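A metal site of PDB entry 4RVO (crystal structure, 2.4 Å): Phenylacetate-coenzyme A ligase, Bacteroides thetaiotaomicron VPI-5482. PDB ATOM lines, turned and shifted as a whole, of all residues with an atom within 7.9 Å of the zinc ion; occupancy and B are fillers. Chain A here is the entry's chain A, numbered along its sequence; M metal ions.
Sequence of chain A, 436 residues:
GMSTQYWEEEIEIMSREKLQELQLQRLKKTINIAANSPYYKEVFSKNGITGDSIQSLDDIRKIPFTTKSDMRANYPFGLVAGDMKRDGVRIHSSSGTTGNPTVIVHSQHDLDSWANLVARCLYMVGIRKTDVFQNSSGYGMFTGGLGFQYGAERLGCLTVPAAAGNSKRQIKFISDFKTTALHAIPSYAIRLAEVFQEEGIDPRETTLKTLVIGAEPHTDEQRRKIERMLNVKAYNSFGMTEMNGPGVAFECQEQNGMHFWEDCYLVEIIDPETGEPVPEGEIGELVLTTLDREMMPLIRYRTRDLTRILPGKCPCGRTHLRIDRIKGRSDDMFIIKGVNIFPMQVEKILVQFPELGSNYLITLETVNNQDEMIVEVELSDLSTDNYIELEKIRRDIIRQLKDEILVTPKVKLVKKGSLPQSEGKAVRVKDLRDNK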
ATOM      1  N   THR A   4      21.955  -2.300  -7.381  1.00  0.00           N
ATOM      2  CA  THR A   4      22.142  -3.128  -8.582  1.00  0.00           C
ATOM      3  C   THR A   4      22.527  -4.578  -8.200  1.00  0.00           C
ATOM      4  O   THR A   4      23.348  -4.774  -7.291  1.00  0.00           O
ATOM      5  CB  THR A   4      23.189  -2.501  -9.525  1.00  0.00           C
ATOM      6  OG1 THR A   4      22.850  -1.127  -9.761  1.00  0.00           O
ATOM      7  CG2 THR A   4      23.300  -3.231 -10.866  1.00  0.00           C
ATOM      8  N   TYR A   6      24.098  -8.358  -9.446  1.00  0.00           N
ATOM      9  CA  TYR A   6      25.010  -8.893 -10.443  1.00  0.00           C
ATOM     10  C   TYR A   6      25.004 -10.427 -10.453  1.00  0.00           C
ATOM     11  O   TYR A   6      24.934 -11.050  -9.397  1.00  0.00           O
ATOM     12  CB  TYR A   6      26.445  -8.384 -10.199  1.00  0.00           C
ATOM     13  CG  TYR A   6      26.535  -6.889  -9.997  1.00  0.00           C
ATOM     14  CD1 TYR A   6      26.628  -6.027 -11.089  1.00  0.00           C
ATOM     15  CD2 TYR A   6      26.570  -6.340  -8.720  1.00  0.00           C
ATOM     16  CE1 TYR A   6      26.703  -4.641 -10.910  1.00  0.00           C
ATOM     17  CE2 TYR A   6      26.643  -4.965  -8.531  1.00  0.00           C
ATOM     18  CZ  TYR A   6      26.704  -4.120  -9.627  1.00  0.00           C
ATOM     19  OH  TYR A   6      26.787  -2.755  -9.437  1.00  0.00           O
ATOM     20  N   MET A 124      21.414  -9.389 -15.848  1.00  0.00           N
ATOM     21  CA  MET A 124      21.742  -7.970 -15.808  1.00  0.00           C
ATOM     22  C   MET A 124      20.511  -7.080 -16.078  1.00  0.00           C
ATOM     23  O   MET A 124      20.365  -6.016 -15.466  1.00  0.00           O
ATOM     24  CB  MET A 124      22.863  -7.649 -16.814  1.00  0.00           C
ATOM     25  CG  MET A 124      23.167  -6.155 -16.938  1.00  0.00           C
ATOM     26  SD  MET A 124      24.817  -5.804 -17.867  1.00  0.00           S
ATOM     27  CE  MET A 124      24.399  -6.589 -19.537  1.00  0.00           C
ATOM     28  N   PHE A 250      25.800  -6.409 -24.389  1.00  0.00           N
ATOM     29  CA  PHE A 250      24.425  -6.312 -23.927  1.00  0.00           C
ATOM     30  C   PHE A 250      24.202  -5.034 -23.131  1.00  0.00           C
ATOM     31  O   PHE A 250      25.044  -4.680 -22.287  1.00  0.00           O
ATOM     32  CB  PHE A 250      24.098  -7.545 -23.048  1.00  0.00           C
ATOM     33  CG  PHE A 250      22.718  -8.140 -23.215  1.00  0.00           C
ATOM     34  CD1 PHE A 250      21.682  -7.763 -22.376  1.00  0.00           C
ATOM     35  CD2 PHE A 250      22.512  -9.204 -24.084  1.00  0.00           C
ATOM     36  CE1 PHE A 250      20.440  -8.390 -22.455  1.00  0.00           C
ATOM     37  CE2 PHE A 250      21.275  -9.852 -24.133  1.00  0.00           C
ATOM     38  CZ  PHE A 250      20.245  -9.435 -23.323  1.00  0.00           C
ATOM     39  N   GLU A 251      23.069  -4.353 -23.340  1.00  0.00           N
ATOM     40  CA  GLU A 251      22.710  -3.164 -22.561  1.00  0.00           C
ATOM     41  C   GLU A 251      22.458  -3.529 -21.104  1.00  0.00           C
ATOM     42  O   GLU A 251      21.983  -4.631 -20.817  1.00  0.00           O
ATOM     43  CB  GLU A 251      21.438  -2.497 -23.131  1.00  0.00           C
ATOM     44  CG  GLU A 251      21.705  -1.497 -24.240  1.00  0.00           C
ATOM     45  CD  GLU A 251      20.456  -0.793 -24.726  1.00  0.00           C
ATOM     46  OE1 GLU A 251      19.371  -1.404 -24.674  1.00  0.00           O
ATOM     47  OE2 GLU A 251      20.571   0.378 -25.158  1.00  0.00           O
ATOM     48  N   CYS A 252      22.708  -2.590 -20.179  1.00  0.00           N
ATOM     49  CA  CYS A 252      22.289  -2.760 -18.792  1.00  0.00           C
ATOM     50  C   CYS A 252      20.914  -2.087 -18.618  1.00  0.00           C
ATOM     51  O   CYS A 252      20.301  -1.684 -19.610  1.00  0.00           O
ATOM     52  CB  CYS A 252      23.324  -2.191 -17.832  1.00  0.00           C
ATOM     53  SG  CYS A 252      23.493  -0.388 -17.900  1.00  0.00           S
ATOM     54  N   GLN A 253      20.425  -1.968 -17.389  1.00  0.00           N
ATOM     55  CA  GLN A 253      19.117  -1.372 -17.147  1.00  0.00           C
ATOM     56  C   GLN A 253      19.145   0.165 -17.386  1.00  0.00           C
ATOM     57  O   GLN A 253      18.083   0.788 -17.476  1.00  0.00           O
ATOM     58  CB  GLN A 253      18.612  -1.696 -15.741  1.00  0.00           C
ATOM     59  CG  GLN A 253      18.388  -3.197 -15.526  1.00  0.00           C
ATOM     60  CD  GLN A 253      17.657  -3.503 -14.239  1.00  0.00           C
ATOM     61  OE1 GLN A 253      16.722  -2.796 -13.838  1.00  0.00           O
ATOM     62  NE2 GLN A 253      17.959  -4.658 -13.654  1.00  0.00           N
ATOM     63  N   GLU A 254      20.351   0.749 -17.614  1.00  0.00           N
ATOM     64  CA  GLU A 254      20.485   2.178 -17.951  1.00  0.00           C
ATOM     65  C   GLU A 254      20.122   2.429 -19.416  1.00  0.00           C
ATOM     66  O   GLU A 254      19.855   3.569 -19.806  1.00  0.00           O
ATOM     67  CB  GLU A 254      21.925   2.687 -17.676  1.00  0.00           C
ATOM     68  CG  GLU A 254      22.296   2.686 -16.198  1.00  0.00           C
ATOM     69  CD  GLU A 254      21.516   3.654 -15.343  1.00  0.00           C
ATOM     70  OE1 GLU A 254      21.259   4.794 -15.812  1.00  0.00           O
ATOM     71  OE2 GLU A 254      21.221   3.307 -14.173  1.00  0.00           O
ATOM     72  N   GLN A 255      20.142   1.347 -20.247  1.00  0.00           N
ATOM     73  CA  GLN A 255      19.823   1.424 -21.688  1.00  0.00           C
ATOM     74  C   GLN A 255      20.663   2.524 -22.382  1.00  0.00           C
ATOM     75  O   GLN A 255      20.146   3.308 -23.178  1.00  0.00           O
ATOM     76  CB  GLN A 255      18.313   1.682 -21.896  1.00  0.00           C
ATOM     77  CG  GLN A 255      17.435   0.527 -21.419  1.00  0.00           C
ATOM     78  CD  GLN A 255      15.976   0.821 -21.611  1.00  0.00           C
ATOM     79  OE1 GLN A 255      15.479   1.897 -21.254  1.00  0.00           O
ATOM     80  NE2 GLN A 255      15.238  -0.148 -22.133  1.00  0.00           N
ATOM     81  N   ASN A 256      21.971   2.571 -22.065  1.00  0.00           N
ATOM     82  CA  ASN A 256      22.889   3.544 -22.660  1.00  0.00           C
ATOM     83  C   ASN A 256      24.221   2.876 -22.970  1.00  0.00           C
ATOM     84  O   ASN A 256      25.111   2.835 -22.112  1.00  0.00           O
ATOM     85  CB  ASN A 256      23.088   4.748 -21.720  1.00  0.00           C
ATOM     86  CG  ASN A 256      23.956   5.845 -22.320  1.00  0.00           C
ATOM     87  OD1 ASN A 256      23.946   6.095 -23.539  1.00  0.00           O
ATOM     88  ND2 ASN A 256      24.662   6.570 -21.461  1.00  0.00           N
ATOM     89  N   GLY A 257      24.317   2.305 -24.171  1.00  0.00           N
ATOM     90  CA  GLY A 257      25.503   1.560 -24.580  1.00  0.00           C
ATOM     91  C   GLY A 257      25.466   0.121 -24.130  1.00  0.00           C
ATOM     92  O   GLY A 257      24.877  -0.191 -23.087  1.00  0.00           O
ATOM     93  N   MET A 258      26.091  -0.766 -24.903  1.00  0.00           N
ATOM     94  CA  MET A 258      26.112  -2.197 -24.587  1.00  0.00           C
ATOM     95  C   MET A 258      27.412  -2.587 -23.911  1.00  0.00           C
ATOM     96  O   MET A 258      28.488  -2.449 -24.511  1.00  0.00           O
ATOM     97  CB  MET A 258      25.901  -3.034 -25.848  1.00  0.00           C
ATOM     98  CG  MET A 258      24.499  -2.970 -26.397  1.00  0.00           C
ATOM     99  SD  MET A 258      24.344  -3.895 -28.065  1.00  0.00           S
ATOM    100  CE  MET A 258      25.171  -2.626 -29.203  1.00  0.00           C
ATOM    101  N   HIS A 259      27.328  -3.111 -22.685  1.00  0.00           N
ATOM    102  CA  HIS A 259      28.505  -3.593 -21.966  1.00  0.00           C
ATOM    103  C   HIS A 259      29.130  -4.782 -22.690  1.00  0.00           C
ATOM    104  O   HIS A 259      28.455  -5.791 -22.932  1.00  0.00           O
ATOM    105  CB  HIS A 259      28.142  -3.979 -20.522  1.00  0.00           C
ATOM    106  CG  HIS A 259      27.909  -2.802 -19.627  1.00  0.00           C
ATOM    107  ND1 HIS A 259      28.970  -2.129 -19.046  1.00  0.00           N
ATOM    108  CD2 HIS A 259      26.755  -2.260 -19.194  1.00  0.00           C
ATOM    109  CE1 HIS A 259      28.425  -1.176 -18.302  1.00  0.00           C
ATOM    110  NE2 HIS A 259      27.087  -1.204 -18.370  1.00  0.00           N
ATOM    111  N   TRP A 261      31.663  -7.856 -22.471  1.00  0.00           N
ATOM    112  CA  TRP A 261      32.277  -8.642 -21.400  1.00  0.00           C
ATOM    113  C   TRP A 261      33.770  -8.861 -21.677  1.00  0.00           C
ATOM    114  O   TRP A 261      34.131  -9.759 -22.454  1.00  0.00           O
ATOM    115  CB  TRP A 261      31.551  -9.974 -21.197  1.00  0.00           C
ATOM    116  CG  TRP A 261      30.110  -9.801 -20.803  1.00  0.00           C
ATOM    117  CD1 TRP A 261      29.018 -10.178 -21.517  1.00  0.00           C
ATOM    118  CD2 TRP A 261      29.619  -9.008 -19.701  1.00  0.00           C
ATOM    119  NE1 TRP A 261      27.867  -9.770 -20.873  1.00  0.00           N
ATOM    120  CE2 TRP A 261      28.213  -9.021 -19.777  1.00  0.00           C
ATOM    121  CE3 TRP A 261      30.242  -8.289 -18.661  1.00  0.00           C
ATOM    122  CZ2 TRP A 261      27.405  -8.383 -18.827  1.00  0.00           C
ATOM    123  CZ3 TRP A 261      29.438  -7.641 -17.730  1.00  0.00           C
ATOM    124  CH2 TRP A 261      28.040  -7.684 -17.815  1.00  0.00           C
ATOM    125  N   LYS A 313      32.027   6.525 -17.016  1.00  0.00           N
ATOM    126  CA  LYS A 313      31.632   5.378 -16.196  1.00  0.00           C
ATOM    127  C   LYS A 313      30.132   5.172 -16.285  1.00  0.00           C
ATOM    128  O   LYS A 313      29.392   6.154 -16.473  1.00  0.00           O
ATOM    129  CB  LYS A 313      32.052   5.594 -14.731  1.00  0.00           C
ATOM    130  CG  LYS A 313      33.548   5.779 -14.541  1.00  0.00           C
ATOM    131  CD  LYS A 313      33.883   6.163 -13.106  1.00  0.00           C
ATOM    132  N   CYS A 314      29.651   3.923 -16.132  1.00  0.00           N
ATOM    133  CA  CYS A 314      28.211   3.681 -16.163  1.00  0.00           C
ATOM    134  C   CYS A 314      27.630   3.713 -14.734  1.00  0.00           C
ATOM    135  O   CYS A 314      28.197   3.114 -13.820  1.00  0.00           O
ATOM    136  CB  CYS A 314      27.882   2.363 -16.858  1.00  0.00           C
ATOM    137  SG  CYS A 314      26.105   2.100 -17.113  1.00  0.00           S
ATOM    138  N   PRO A 315      26.410   4.294 -14.562  1.00  0.00           N
ATOM    139  CA  PRO A 315      25.821   4.368 -13.204  1.00  0.00           C
ATOM    140  C   PRO A 315      25.459   2.982 -12.623  1.00  0.00           C
ATOM    141  O   PRO A 315      25.219   2.881 -11.414  1.00  0.00           O
ATOM    142  CB  PRO A 315      24.558   5.209 -13.409  1.00  0.00           C
ATOM    143  CG  PRO A 315      24.805   5.972 -14.663  1.00  0.00           C
ATOM    144  CD  PRO A 315      25.623   5.081 -15.533  1.00  0.00           C
ATOM    145  N   CYS A 316      25.411   1.906 -13.472  1.00  0.00           N
ATOM    146  CA  CYS A 316      25.070   0.559 -12.959  1.00  0.00           C
ATOM    147  C   CYS A 316      26.253  -0.025 -12.118  1.00  0.00           C
ATOM    148  O   CYS A 316      26.067  -0.995 -11.392  1.00  0.00           O
ATOM    149  CB  CYS A 316      24.687  -0.377 -14.111  1.00  0.00           C
ATOM    150  SG  CYS A 316      26.088  -1.030 -15.048  1.00  0.00           S
ATOM    151  N   GLY A 317      27.427   0.610 -12.219  1.00  0.00           N
ATOM    152  CA  GLY A 317      28.594   0.229 -11.439  1.00  0.00           C
ATOM    153  C   GLY A 317      29.538  -0.725 -12.142  1.00  0.00           C
ATOM    154  O   GLY A 317      30.639  -0.986 -11.653  1.00  0.00           O
ATOM    155  N   ARG A 318      29.116  -1.266 -13.307  1.00  0.00           N
ATOM    156  CA  ARG A 318      29.934  -2.209 -14.047  1.00  0.00           C
ATOM    157  C   ARG A 318      31.097  -1.504 -14.743  1.00  0.00           C
ATOM    158  O   ARG A 318      30.935  -0.381 -15.250  1.00  0.00           O
ATOM    159  CB  ARG A 318      29.098  -3.003 -15.044  1.00  0.00           C
ATOM    160  CG  ARG A 318      28.157  -4.006 -14.372  1.00  0.00           C
ATOM    161  CD  ARG A 318      27.248  -4.684 -15.357  1.00  0.00           C
ATOM    162  NE  ARG A 318      26.325  -5.617 -14.703  1.00  0.00           N
ATOM    163  CZ  ARG A 318      25.129  -5.273 -14.226  1.00  0.00           C
ATOM    164  NH1 ARG A 318      24.703  -4.015 -14.323  1.00  0.00           N
ATOM    165  NH2 ARG A 318      24.359  -6.176 -13.643  1.00  0.00           N
ATOM    166  N   THR A 319      32.296  -2.118 -14.686  1.00  0.00           N
ATOM    167  CA  THR A 319      33.527  -1.511 -15.183  1.00  0.00           C
ATOM    168  C   THR A 319      33.827  -1.933 -16.629  1.00  0.00           C
ATOM    169  O   THR A 319      34.755  -1.402 -17.245  1.00  0.00           O
ATOM    170  CB  THR A 319      34.687  -1.884 -14.263  1.00  0.00           C
ATOM    171  OG1 THR A 319      34.686  -3.311 -14.090  1.00  0.00           O
ATOM    172  CG2 THR A 319      34.600  -1.197 -12.899  1.00  0.00           C
ATOM    173  N   HIS A 320      33.079  -2.911 -17.153  1.00  0.00           N
ATOM    174  CA  HIS A 320      33.275  -3.386 -18.522  1.00  0.00           C
ATOM    175  C   HIS A 320      32.846  -2.315 -19.517  1.00  0.00           C
ATOM    176  O   HIS A 320      31.811  -1.678 -19.331  1.00  0.00           O
ATOM    177  CB  HIS A 320      32.505  -4.688 -18.757  1.00  0.00           C
ATOM    178  CG  HIS A 320      33.033  -5.834 -17.952  1.00  0.00           C
ATOM    179  ND1 HIS A 320      33.837  -6.809 -18.522  1.00  0.00           N
ATOM    180  CD2 HIS A 320      32.939  -6.078 -16.625  1.00  0.00           C
ATOM    181  CE1 HIS A 320      34.146  -7.630 -17.541  1.00  0.00           C
ATOM    182  NE2 HIS A 320      33.638  -7.228 -16.383  1.00  0.00           N
ATOM    183  N   ARG A 322      31.537   0.030 -22.701  1.00  0.00           N
ATOM    184  CA  ARG A 322      30.277   0.057 -23.434  1.00  0.00           C
ATOM    185  C   ARG A 322      30.509   0.503 -24.853  1.00  0.00           C
ATOM    186  O   ARG A 322      31.211   1.486 -25.082  1.00  0.00           O
ATOM    187  CB  ARG A 322      29.272   1.005 -22.738  1.00  0.00           C
ATOM    188  CG  ARG A 322      28.841   0.535 -21.364  1.00  0.00           C
ATOM    189  CD  ARG A 322      28.071   1.604 -20.608  1.00  0.00           C
ATOM    190  NE  ARG A 322      28.902   2.770 -20.305  1.00  0.00           N
ATOM    191  CZ  ARG A 322      28.742   3.965 -20.862  1.00  0.00           C
ATOM    192  NH1 ARG A 322      27.741   4.174 -21.702  1.00  0.00           N
ATOM    193  NH2 ARG A 322      29.546   4.962 -20.533  1.00  0.00           N
HETATM  194 ZN    ZN M   1      25.754  -0.330 -17.111  1.00  0.00          ZN
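The side-chain sulfur (SG) of Cys 316 lies close to the guanidinium group (NH1) of Arg 318 (3.4 Å). O of Cys 316 lies within hydrogen-bond range of OH of Tyr 6 (2.7 Å). N of Glu 254 sits close to SG of Cys 252 (3.4 Å). ND1 of His 259 lies within hydrogen-bond range of O of His 320, at 2.9 Å. O of Phe 250 is in hydrogen-bond range of N of His 259, 2.8 Å away.
The zinc ion is bound by a ring nitrogen (NE2) of His 259 (2.0 Å), the side-chain sulfur (SG) of Cys 316 (2.2 Å), the side-chain sulfur (SG) of Cys 252 (2.4 Å) and the side-chain sulfur (SG) of Cys 314 (2.5 Å).
Along chain A the residues within 4 Å of the zinc ion span positions 252 to 316. The nearest printed residue that does not touch the zinc ion is Arg 322 (4.6 Å).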
